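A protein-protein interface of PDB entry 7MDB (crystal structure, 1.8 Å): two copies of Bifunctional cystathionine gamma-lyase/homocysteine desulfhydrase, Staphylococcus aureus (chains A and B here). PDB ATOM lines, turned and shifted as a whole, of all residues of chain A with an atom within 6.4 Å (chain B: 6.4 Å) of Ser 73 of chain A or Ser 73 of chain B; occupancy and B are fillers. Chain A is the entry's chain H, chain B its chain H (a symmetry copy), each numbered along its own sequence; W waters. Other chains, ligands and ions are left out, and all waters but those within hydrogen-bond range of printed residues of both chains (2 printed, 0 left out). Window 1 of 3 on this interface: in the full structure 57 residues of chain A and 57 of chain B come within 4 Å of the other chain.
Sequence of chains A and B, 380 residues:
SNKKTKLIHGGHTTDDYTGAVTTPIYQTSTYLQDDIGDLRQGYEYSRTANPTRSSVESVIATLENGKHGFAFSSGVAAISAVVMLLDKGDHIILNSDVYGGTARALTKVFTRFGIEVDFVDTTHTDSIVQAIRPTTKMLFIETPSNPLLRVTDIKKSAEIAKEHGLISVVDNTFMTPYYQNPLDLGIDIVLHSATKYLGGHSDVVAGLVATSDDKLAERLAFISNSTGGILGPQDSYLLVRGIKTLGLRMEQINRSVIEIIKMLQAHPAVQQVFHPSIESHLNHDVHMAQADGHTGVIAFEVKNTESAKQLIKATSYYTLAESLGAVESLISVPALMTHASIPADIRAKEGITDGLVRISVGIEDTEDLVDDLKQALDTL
Ser 73 of chain A touches Gly 228 of chain B, and with the chains exchanged Gly 228 of chain A touches Ser 73 of chain B.
Ser 73 of chain A touches Gly 229 of chain B, and with the chains exchanged Gly 229 of chain A touches Ser 73 of chain B.
Ser 73 of chain A touches Ile 230 of chain B, and with the chains exchanged Ile 230 of chain A touches Ser 73 of chain B.
Ala 77 of chain A touches Thr 227 of chain B, and with the chains exchanged Thr 227 of chain A touches Ala 77 of chain B.
Positions printed for both chains: 71, 72, 73, 74, 75, 77, 78, 195, 196, 205, 206, 207, 227, 228, 229, 230, 231 and 232.
Of the 13 pairs that touch across the chains among the printed residues, 13 have their exchanged pair printed and touching as well.
N of Ala 77 of chain A sits close to O of Thr 227 of chain B (3.4 Å).
O of Thr 227 of chain A lies close to N of Ala 77 of chain B.
OG of Ser 73 of chain A is in hydrogen-bond range of O of Gly 228 of chain B (2.9 Å).
O of Gly 228 of chain A sits at hydrogen-bond distance from OG of Ser 74 of chain B (2.8 Å).
O of Gly 228 of chain A sits at hydrogen-bond distance from OG of Ser 73 of chain B (2.9 Å).
The backbone carbonyl oxygen (O) of Gly 228 of chain B lies within hydrogen-bond range of the side-chain hydroxyl (OG) of Ser 74 of chain A (2.8 Å).
Water W2 bridges the backbone carbonyl oxygen of Ile 230 of chain A (2.9 Å) and the backbone carbonyl oxygen of Ser 73 of chain B (3.1 Å).
Water W1 lies within hydrogen-bond range of O of Ile 230 of chain B and O of Ser 73 of chain A.
Printed residues of chain B within 4 Å of Ser 74 of chain A: Gly 228.
Of the printed residues of chain B, Ala 77 of chain A touches Thr 227 (3.1 Å) and Gly 228 (3.5 Å).
Ala 78 of chain A touches none of the printed residues of chain B.
Ser 73 of chain B touches just these residues of chain A: Ser 73, Gly 228, Gly 229 and Ile 230.
Printed residues of chain A within 4 Å of Ser 74 of chain B: Gly 228.
LLP 196 of chain B touches none of the printed residues of chain A.
The nearest residue of chain B that does not touch Ser 73 of chain A is Thr 227 of chain B (5.6 Å).
The nearest residue of chain A that does not touch Ser 73 of chain B is Thr 227 of chain A (5.6 Å).
OG of Ser 73 of chain A touches OG of Ser 73 of chain B, 3.8 Å away.
Ser 73 of chain A touches Gly 229 of chain B.
Ser 73 of chain A touches Ile 230 of chain B (CB to O, 3.5 Å).
CB of Ala 77 of chain A touches O of Gly 228 of chain B (3.5 Å).
Gly 228 of chain A touches Ala 77 of chain B.
CA of Gly 229 of chain A touches OG of Ser 73 of chain B (3.3 Å).
CB of Ser 73 of chain B touches O of Ile 230 of chain A, 3.5 Å away.
The side-chain hydroxyl of Ser 74 of chain B lies within hydrogen-bond range of the backbone NH of Ala 77 of chain B (3.1 Å).
N of Ser 73 of chain B sits at hydrogen-bond distance from O of Gly 229 of chain B (2.9 Å).
OG of Ser 74 of chain A is in hydrogen-bond range of N of Ala 77 of chain A (3.1 Å).
O of Ser 74 of chain A lies close to N of Gly 207 of chain A, at 3.3 Å.
The backbone NH (N) of Gly 207 of chain B sits close to the backbone carbonyl oxygen (O) of Ser 74 of chain B (3.3 Å).
N of Ser 73 of chain A lies within hydrogen-bond range of O of Gly 229 of chain A (2.9 Å).
Of the 18 printed residues of chain B, 7 touch a printed residue of chain A.
Printed residues of chain B that touch a printed residue of chain A: Ser 73, Ser 74, Ala 77, Thr 227, Gly 228, Gly 229 and Ile 230.
Hydrophobic or aromatic side chains of chain B within 4 Å of the printed part of chain A: Ala 77 and Ile 230.
Printed residues of chain A that touch a printed residue of chain B: Ser 73, Ser 74, Ala 77, Thr 227, Gly 228, Gly 229 and Ile 230.
Hydrophobic or aromatic side chains of chain A within 4 Å of the printed part of chain B: Ala 77 and Ile 230.
Among the printed residues, no Asp or Glu carboxylate lies within 4 Å of a Lys or Arg side-chain nitrogen of the other chain.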
ATOM      1  N   ALA A  71      17.046  10.022   7.925  1.00  0.00           N
ATOM      2  CA  ALA A  71      18.186   9.178   7.590  1.00  0.00           C
ATOM      3  C   ALA A  71      18.079   7.858   8.340  1.00  0.00           C
ATOM      4  O   ALA A  71      17.944   7.834   9.571  1.00  0.00           O
ATOM      5  CB  ALA A  71      19.520   9.882   7.913  1.00  0.00           C
ATOM      6  N   PHE A  72      18.162   6.764   7.595  1.00  0.00           N
ATOM      7  CA  PHE A  72      17.992   5.425   8.118  1.00  0.00           C
ATOM      8  C   PHE A  72      19.264   4.613   7.899  1.00  0.00           C
ATOM      9  O   PHE A  72      20.111   4.951   7.065  1.00  0.00           O
ATOM     10  CB  PHE A  72      16.796   4.735   7.438  1.00  0.00           C
ATOM     11  CG  PHE A  72      15.472   5.351   7.787  1.00  0.00           C
ATOM     12  CD1 PHE A  72      14.951   6.388   7.025  1.00  0.00           C
ATOM     13  CD2 PHE A  72      14.764   4.913   8.896  1.00  0.00           C
ATOM     14  CE1 PHE A  72      13.737   6.967   7.362  1.00  0.00           C
ATOM     15  CE2 PHE A  72      13.546   5.491   9.237  1.00  0.00           C
ATOM     16  CZ  PHE A  72      13.041   6.514   8.466  1.00  0.00           C
ATOM     17  N   SER A  73      19.358   3.502   8.632  1.00  0.00           N
ATOM     18  CA  SER A  73      20.554   2.670   8.630  1.00  0.00           C
ATOM     19  C   SER A  73      20.780   1.930   7.308  1.00  0.00           C
ATOM     20  O   SER A  73      21.821   1.283   7.160  1.00  0.00           O
ATOM     21  CB  SER A  73      20.463   1.661   9.774  1.00  0.00           C
ATOM     22  OG  SER A  73      19.153   1.100   9.818  1.00  0.00           O
ATOM     23  N   SER A  74      19.827   1.972   6.373  1.00  0.00           N
ATOM     24  CA  SER A  74      19.956   1.361   5.052  1.00  0.00           C
ATOM     25  C   SER A  74      18.765   1.794   4.214  1.00  0.00           C
ATOM     26  O   SER A  74      17.751   2.270   4.740  1.00  0.00           O
ATOM     27  CB  SER A  74      19.997  -0.175   5.124  1.00  0.00           C
ATOM     28  OG  SER A  74      18.771  -0.677   5.676  1.00  0.00           O
ATOM     29  N   GLY A  75      18.885   1.588   2.903  1.00  0.00           N
ATOM     30  CA  GLY A  75      17.736   1.791   2.036  1.00  0.00           C
ATOM     31  C   GLY A  75      16.532   0.953   2.439  1.00  0.00           C
ATOM     32  O   GLY A  75      15.394   1.448   2.468  1.00  0.00           O
ATOM     33  N   ALA A  77      15.779  -0.117   5.340  1.00  0.00           N
ATOM     34  CA  ALA A  77      15.199   0.407   6.576  1.00  0.00           C
ATOM     35  C   ALA A  77      14.320   1.617   6.294  1.00  0.00           C
ATOM     36  O   ALA A  77      13.260   1.773   6.911  1.00  0.00           O
ATOM     37  CB  ALA A  77      16.297   0.750   7.592  1.00  0.00           C
ATOM     38  N   ALA A  78      14.725   2.469   5.347  1.00  0.00           N
ATOM     39  CA  ALA A  78      13.867   3.580   4.945  1.00  0.00           C
ATOM     40  C   ALA A  78      12.567   3.073   4.331  1.00  0.00           C
ATOM     41  O   ALA A  78      11.473   3.575   4.642  1.00  0.00           O
ATOM     42  CB  ALA A  78      14.597   4.475   3.953  1.00  0.00           C
ATOM     43  N   THR A 195      23.209   4.242  -0.071  1.00  0.00           N
ATOM     44  CA  THR A 195      24.298   3.296  -0.286  1.00  0.00           C
ATOM     45  C   THR A 195      24.874   3.415  -1.700  1.00  0.00           C
ATOM     46  O   THR A 195      26.047   3.098  -1.938  1.00  0.00           O
ATOM     47  CB  THR A 195      23.790   1.835  -0.051  1.00  0.00           C
ATOM     48  OG1 THR A 195      23.108   1.773   1.207  1.00  0.00           O
ATOM     49  CG2 THR A 195      24.948   0.816  -0.049  1.00  0.00           C
ATOM     50  N1  LLP A 196      16.170   0.345  -3.747  1.00  0.00           N
ATOM     51  C2  LLP A 196      17.022   0.431  -4.740  1.00  0.00           C
ATOM     52  C2' LLP A 196      16.514   0.968  -6.043  1.00  0.00           C
ATOM     53  C3  LLP A 196      18.367   0.049  -4.593  1.00  0.00           C
ATOM     54  O3  LLP A 196      19.226   0.162  -5.685  1.00  0.00           O
ATOM     55  C4  LLP A 196      18.820  -0.450  -3.374  1.00  0.00           C
ATOM     56  C4' LLP A 196      20.249  -0.830  -3.216  1.00  0.00           C
ATOM     57  C5  LLP A 196      17.860  -0.546  -2.318  1.00  0.00           C
ATOM     58  C6  LLP A 196      16.570  -0.125  -2.591  1.00  0.00           C
ATOM     59  C5' LLP A 196      18.135  -1.089  -0.924  1.00  0.00           C
ATOM     60  OP4 LLP A 196      18.971  -0.223  -0.243  1.00  0.00           O
ATOM     61  P   LLP A 196      20.028  -0.778   0.852  1.00  0.00           P
ATOM     62  OP1 LLP A 196      20.851  -1.851   0.170  1.00  0.00           O
ATOM     63  OP2 LLP A 196      20.839   0.434   1.270  1.00  0.00           O
ATOM     64  OP3 LLP A 196      19.245  -1.358   2.008  1.00  0.00           O
ATOM     65  N   LLP A 196      24.043   3.867  -2.636  1.00  0.00           N
ATOM     66  CA  LLP A 196      24.427   3.896  -4.036  1.00  0.00           C
ATOM     67  CB  LLP A 196      23.217   3.540  -4.919  1.00  0.00           C
ATOM     68  CG  LLP A 196      22.407   2.362  -4.341  1.00  0.00           C
ATOM     69  CD  LLP A 196      23.222   1.071  -4.230  1.00  0.00           C
ATOM     70  CE  LLP A 196      22.489  -0.032  -3.431  1.00  0.00           C
ATOM     71  NZ  LLP A 196      21.207  -0.443  -4.005  1.00  0.00           N
ATOM     72  C   LLP A 196      25.019   5.268  -4.400  1.00  0.00           C
ATOM     73  O   LLP A 196      26.079   5.634  -3.839  1.00  0.00           O
ATOM     74  N   VAL A 205      26.360   2.261   4.046  1.00  0.00           N
ATOM     75  CA  VAL A 205      25.028   1.699   3.828  1.00  0.00           C
ATOM     76  C   VAL A 205      24.036   2.618   4.536  1.00  0.00           C
ATOM     77  O   VAL A 205      24.177   2.874   5.736  1.00  0.00           O
ATOM     78  CB  VAL A 205      24.932   0.253   4.342  1.00  0.00           C
ATOM     79  CG1 VAL A 205      23.501  -0.268   4.206  1.00  0.00           C
ATOM     80  CG2 VAL A 205      25.897  -0.644   3.577  1.00  0.00           C
ATOM     81  N   ALA A 206      23.050   3.130   3.801  1.00  0.00           N
ATOM     82  CA  ALA A 206      22.191   4.182   4.343  1.00  0.00           C
ATOM     83  C   ALA A 206      20.938   4.342   3.495  1.00  0.00           C
ATOM     84  O   ALA A 206      20.955   4.104   2.282  1.00  0.00           O
ATOM     85  CB  ALA A 206      22.941   5.527   4.401  1.00  0.00           C
ATOM     86  N   GLY A 207      19.861   4.792   4.141  1.00  0.00           N
ATOM     87  CA  GLY A 207      18.653   5.193   3.442  1.00  0.00           C
ATOM     88  C   GLY A 207      18.317   6.641   3.751  1.00  0.00           C
ATOM     89  O   GLY A 207      18.628   7.142   4.828  1.00  0.00           O
ATOM     90  N   THR A 227      11.012   2.445  16.165  1.00  0.00           N
ATOM     91  CA  THR A 227      11.627   1.224  15.661  1.00  0.00           C
ATOM     92  C   THR A 227      13.123   1.384  15.402  1.00  0.00           C
ATOM     93  O   THR A 227      13.799   0.381  15.170  1.00  0.00           O
ATOM     94  CB  THR A 227      10.921   0.730  14.384  1.00  0.00           C
ATOM     95  OG1 THR A 227      10.947   1.746  13.375  1.00  0.00           O
ATOM     96  CG2 THR A 227       9.444   0.353  14.684  1.00  0.00           C
ATOM     97  N   GLY A 228      13.638   2.610  15.412  1.00  0.00           N
ATOM     98  CA  GLY A 228      15.050   2.855  15.668  1.00  0.00           C
ATOM     99  C   GLY A 228      16.040   2.501  14.577  1.00  0.00           C
ATOM    100  O   GLY A 228      17.223   2.320  14.882  1.00  0.00           O
ATOM    101  N   GLY A 229      15.612   2.426  13.321  1.00  0.00           N
ATOM    102  CA  GLY A 229      16.520   2.146  12.223  1.00  0.00           C
ATOM    103  C   GLY A 229      17.275   3.382  11.750  1.00  0.00           C
ATOM    104  O   GLY A 229      17.257   3.703  10.560  1.00  0.00           O
ATOM    105  N   ILE A 230      17.963   4.080  12.673  1.00  0.00           N
ATOM    106  CA  ILE A 230      18.542   5.391  12.393  1.00  0.00           C
ATOM    107  C   ILE A 230      19.949   5.228  11.836  1.00  0.00           C
ATOM    108  O   ILE A 230      20.688   4.313  12.202  1.00  0.00           O
ATOM    109  CB  ILE A 230      18.571   6.271  13.662  1.00  0.00           C
ATOM    110  CG1 ILE A 230      19.243   5.495  14.801  1.00  0.00           C
ATOM    111  CG2 ILE A 230      17.158   6.655  14.066  1.00  0.00           C
ATOM    112  CD1 ILE A 230      20.088   6.336  15.707  1.00  0.00           C
ATOM    113  N   LEU A 231      20.344   6.161  10.983  1.00  0.00           N
ATOM    114  CA  LEU A 231      21.736   6.233  10.545  1.00  0.00           C
ATOM    115  C   LEU A 231      22.619   6.840  11.636  1.00  0.00           C
ATOM    116  O   LEU A 231      22.247   7.829  12.282  1.00  0.00           O
ATOM    117  CB  LEU A 231      21.830   7.057   9.257  1.00  0.00           C
ATOM    118  CG  LEU A 231      23.178   6.995   8.520  1.00  0.00           C
ATOM    119  CD1 LEU A 231      23.435   5.569   8.022  1.00  0.00           C
ATOM    120  CD2 LEU A 231      23.212   7.970   7.367  1.00  0.00           C
ATOM    121  N   GLY A 232      23.808   6.250  11.838  1.00  0.00           N
ATOM    122  CA  GLY A 232      24.761   6.775  12.805  1.00  0.00           C
ATOM    123  C   GLY A 232      25.471   8.016  12.297  1.00  0.00           C
ATOM    124  O   GLY A 232      25.400   8.386  11.117  1.00  0.00           O
ATOM    125  N   ALA B  71      23.785  -7.204  15.553  1.00  0.00           N
ATOM    126  CA  ALA B  71      23.986  -5.814  15.939  1.00  0.00           C
ATOM    127  C   ALA B  71      23.036  -4.925  15.149  1.00  0.00           C
ATOM    128  O   ALA B  71      23.003  -4.969  13.911  1.00  0.00           O
ATOM    129  CB  ALA B  71      25.449  -5.376  15.723  1.00  0.00           C
ATOM    130  N   PHE B  72      22.282  -4.104  15.868  1.00  0.00           N
ATOM    131  CA  PHE B  72      21.260  -3.252  15.299  1.00  0.00           C
ATOM    132  C   PHE B  72      21.584  -1.789  15.580  1.00  0.00           C
ATOM    133  O   PHE B  72      22.369  -1.461  16.475  1.00  0.00           O
ATOM    134  CB  PHE B  72      19.880  -3.613  15.882  1.00  0.00           C
ATOM    135  CG  PHE B  72      19.391  -4.969  15.463  1.00  0.00           C
ATOM    136  CD1 PHE B  72      19.695  -6.095  16.217  1.00  0.00           C
ATOM    137  CD2 PHE B  72      18.653  -5.121  14.299  1.00  0.00           C
ATOM    138  CE1 PHE B  72      19.256  -7.347  15.817  1.00  0.00           C
ATOM    139  CE2 PHE B  72      18.211  -6.376  13.895  1.00  0.00           C
ATOM    140  CZ  PHE B  72      18.516  -7.481  14.658  1.00  0.00           C
ATOM    141  N   SER B  73      20.923  -0.909  14.825  1.00  0.00           N
ATOM    142  CA  SER B  73      21.193   0.521  14.883  1.00  0.00           C
ATOM    143  C   SER B  73      20.750   1.173  16.197  1.00  0.00           C
ATOM    144  O   SER B  73      21.030   2.359  16.395  1.00  0.00           O
ATOM    145  CB  SER B  73      20.497   1.210  13.709  1.00  0.00           C
ATOM    146  OG  SER B  73      19.175   0.696  13.564  1.00  0.00           O
ATOM    147  N   SER B  74      20.040   0.452  17.068  1.00  0.00           N
ATOM    148  CA  SER B  74      19.618   0.944  18.378  1.00  0.00           C
ATOM    149  C   SER B  74      19.018  -0.220  19.148  1.00  0.00           C
ATOM    150  O   SER B  74      18.663  -1.255  18.570  1.00  0.00           O
ATOM    151  CB  SER B  74      18.580   2.072  18.268  1.00  0.00           C
ATOM    152  OG  SER B  74      17.391   1.589  17.624  1.00  0.00           O
ATOM    153  N   GLY B  75      18.874  -0.024  20.458  1.00  0.00           N
ATOM    154  CA  GLY B  75      18.141  -0.995  21.253  1.00  0.00           C
ATOM    155  C   GLY B  75      16.724  -1.227  20.750  1.00  0.00           C
ATOM    156  O   GLY B  75      16.261  -2.374  20.660  1.00  0.00           O
ATOM    157  N   ALA B  77      15.629  -0.911  17.779  1.00  0.00           N
ATOM    158  CA  ALA B  77      15.663  -1.658  16.522  1.00  0.00           C
ATOM    159  C   ALA B  77      15.864  -3.144  16.778  1.00  0.00           C
ATOM    160  O   ALA B  77      15.258  -3.980  16.097  1.00  0.00           O
ATOM    161  CB  ALA B  77      16.750  -1.108  15.590  1.00  0.00           C
ATOM    162  N   ALA B  78      16.686  -3.496  17.772  1.00  0.00           N
ATOM    163  CA  ALA B  78      16.824  -4.900  18.147  1.00  0.00           C
ATOM    164  C   ALA B  78      15.504  -5.462  18.661  1.00  0.00           C
ATOM    165  O   ALA B  78      15.096  -6.577  18.293  1.00  0.00           O
ATOM    166  CB  ALA B  78      17.905  -5.056  19.208  1.00  0.00           C
ATOM    167  N   THR B 195      23.614   1.021  23.777  1.00  0.00           N
ATOM    168  CA  THR B 195      23.716   2.453  24.037  1.00  0.00           C
ATOM    169  C   THR B 195      24.117   2.732  25.488  1.00  0.00           C
ATOM    170  O   THR B 195      24.715   3.773  25.794  1.00  0.00           O
ATOM    171  CB  THR B 195      22.348   3.148  23.731  1.00  0.00           C
ATOM    172  OG1 THR B 195      21.901   2.750  22.430  1.00  0.00           O
ATOM    173  CG2 THR B 195      22.461   4.686  23.777  1.00  0.00           C
ATOM    174  N1  LLP B 196      15.637  -1.209  26.881  1.00  0.00           N
ATOM    175  C2  LLP B 196      16.240  -0.702  27.930  1.00  0.00           C
ATOM    176  C2' LLP B 196      16.168  -1.476  29.210  1.00  0.00           C
ATOM    177  C3  LLP B 196      16.941   0.515  27.861  1.00  0.00           C
ATOM    178  O3  LLP B 196      17.561   1.005  29.009  1.00  0.00           O
ATOM    179  C4  LLP B 196      16.994   1.220  26.661  1.00  0.00           C
ATOM    180  C4' LLP B 196      17.757   2.495  26.586  1.00  0.00           C
ATOM    181  C5  LLP B 196      16.312   0.646  25.542  1.00  0.00           C
ATOM    182  C6  LLP B 196      15.670  -0.563  25.741  1.00  0.00           C
ATOM    183  C5' LLP B 196      16.220   1.264  24.155  1.00  0.00           C
ATOM    184  OP4 LLP B 196      17.465   1.246  23.554  1.00  0.00           O
ATOM    185  P   LLP B 196      17.901   2.411  22.516  1.00  0.00           P
ATOM    186  OP1 LLP B 196      17.693   3.735  23.220  1.00  0.00           O
ATOM    187  OP2 LLP B 196      19.353   2.122  22.184  1.00  0.00           O
ATOM    188  OP3 LLP B 196      17.013   2.310  21.296  1.00  0.00           O
ATOM    189  N   LLP B 196      23.779   1.804  26.380  1.00  0.00           N
ATOM    190  CA  LLP B 196      23.982   2.014  27.802  1.00  0.00           C
ATOM    191  CB  LLP B 196      22.814   1.400  28.595  1.00  0.00           C
ATOM    192  CG  LLP B 196      21.451   1.691  27.934  1.00  0.00           C
ATOM    193  CD  LLP B 196      21.138   3.186  27.842  1.00  0.00           C
ATOM    194  CE  LLP B 196      19.896   3.483  26.967  1.00  0.00           C
ATOM    195  NZ  LLP B 196      18.658   2.866  27.446  1.00  0.00           N
ATOM    196  C   LLP B 196      25.339   1.437  28.240  1.00  0.00           C
ATOM    197  O   LLP B 196      26.386   1.932  27.760  1.00  0.00           O
ATOM    198  N   VAL B 205      24.744   4.748  19.824  1.00  0.00           N
ATOM    199  CA  VAL B 205      23.388   4.214  19.939  1.00  0.00           C
ATOM    200  C   VAL B 205      23.370   2.883  19.192  1.00  0.00           C
ATOM    201  O   VAL B 205      23.727   2.830  18.011  1.00  0.00           O
ATOM    202  CB  VAL B 205      22.343   5.194  19.381  1.00  0.00           C
ATOM    203  CG1 VAL B 205      20.951   4.563  19.410  1.00  0.00           C
ATOM    204  CG2 VAL B 205      22.353   6.489  20.183  1.00  0.00           C
ATOM    205  N   ALA B 206      22.977   1.808  19.875  1.00  0.00           N
ATOM    206  CA  ALA B 206      23.136   0.470  19.306  1.00  0.00           C
ATOM    207  C   ALA B 206      22.300  -0.542  20.074  1.00  0.00           C
ATOM    208  O   ALA B 206      22.066  -0.392  21.280  1.00  0.00           O
ATOM    209  CB  ALA B 206      24.614   0.034  19.333  1.00  0.00           C
ATOM    210  N   GLY B 207      21.889  -1.600  19.372  1.00  0.00           N
ATOM    211  CA  GLY B 207      21.263  -2.749  20.001  1.00  0.00           C
ATOM    212  C   GLY B 207      22.056  -4.010  19.709  1.00  0.00           C
ATOM    213  O   GLY B 207      22.698  -4.123  18.668  1.00  0.00           O
ATOM    214  N   THR B 227      14.730  -5.785   6.738  1.00  0.00           N
ATOM    215  CA  THR B 227      14.282  -4.496   7.248  1.00  0.00           C
ATOM    216  C   THR B 227      15.442  -3.572   7.608  1.00  0.00           C
ATOM    217  O   THR B 227      15.208  -2.388   7.857  1.00  0.00           O
ATOM    218  CB  THR B 227      13.350  -4.670   8.463  1.00  0.00           C
ATOM    219  OG1 THR B 227      14.013  -5.405   9.498  1.00  0.00           O
ATOM    220  CG2 THR B 227      12.054  -5.425   8.058  1.00  0.00           C
ATOM    221  N   GLY B 228      16.667  -4.088   7.665  1.00  0.00           N
ATOM    222  CA  GLY B 228      17.860  -3.270   7.508  1.00  0.00           C
ATOM    223  C   GLY B 228      18.247  -2.354   8.651  1.00  0.00           C
ATOM    224  O   GLY B 228      18.983  -1.390   8.420  1.00  0.00           O
ATOM    225  N   GLY B 229      17.807  -2.633   9.875  1.00  0.00           N
ATOM    226  CA  GLY B 229      18.187  -1.828  11.022  1.00  0.00           C
ATOM    227  C   GLY B 229      19.558  -2.196  11.576  1.00  0.00           C
ATOM    228  O   GLY B 229      19.691  -2.470  12.770  1.00  0.00           O
ATOM    229  N   ILE B 230      20.595  -2.190  10.718  1.00  0.00           N
ATOM    230  CA  ILE B 230      21.906  -2.730  11.071  1.00  0.00           C
ATOM    231  C   ILE B 230      22.758  -1.645  11.713  1.00  0.00           C
ATOM    232  O   ILE B 230      22.669  -0.465  11.372  1.00  0.00           O
ATOM    233  CB  ILE B 230      22.624  -3.305   9.830  1.00  0.00           C
ATOM    234  CG1 ILE B 230      22.635  -2.250   8.717  1.00  0.00           C
ATOM    235  CG2 ILE B 230      21.913  -4.556   9.344  1.00  0.00           C
ATOM    236  CD1 ILE B 230      23.884  -2.237   7.890  1.00  0.00           C
ATOM    237  N   LEU B 231      23.636  -2.058  12.615  1.00  0.00           N
ATOM    238  CA  LEU B 231      24.649  -1.149  13.144  1.00  0.00           C
ATOM    239  C   LEU B 231      25.773  -0.937  12.130  1.00  0.00           C
ATOM    240  O   LEU B 231      26.242  -1.886  11.488  1.00  0.00           O
ATOM    241  CB  LEU B 231      25.208  -1.706  14.457  1.00  0.00           C
ATOM    242  CG  LEU B 231      26.077  -0.740  15.278  1.00  0.00           C
ATOM    243  CD1 LEU B 231      25.231   0.446  15.755  1.00  0.00           C
ATOM    244  CD2 LEU B 231      26.707  -1.444  16.457  1.00  0.00           C
ATOM    245  N   GLY B 232      26.222   0.321  11.990  1.00  0.00           N
ATOM    246  CA  GLY B 232      27.331   0.637  11.101  1.00  0.00           C
ATOM    247  C   GLY B 232      28.671   0.233  11.687  1.00  0.00           C
ATOM    248  O   GLY B 232      28.801  -0.113  12.870  1.00  0.00           O
HETATM  249  O   HOH W   1      23.706   1.513   9.569  1.00  0.00           O
HETATM  250  O   HOH W   2      22.691   3.576  14.120  1.00  0.00           O
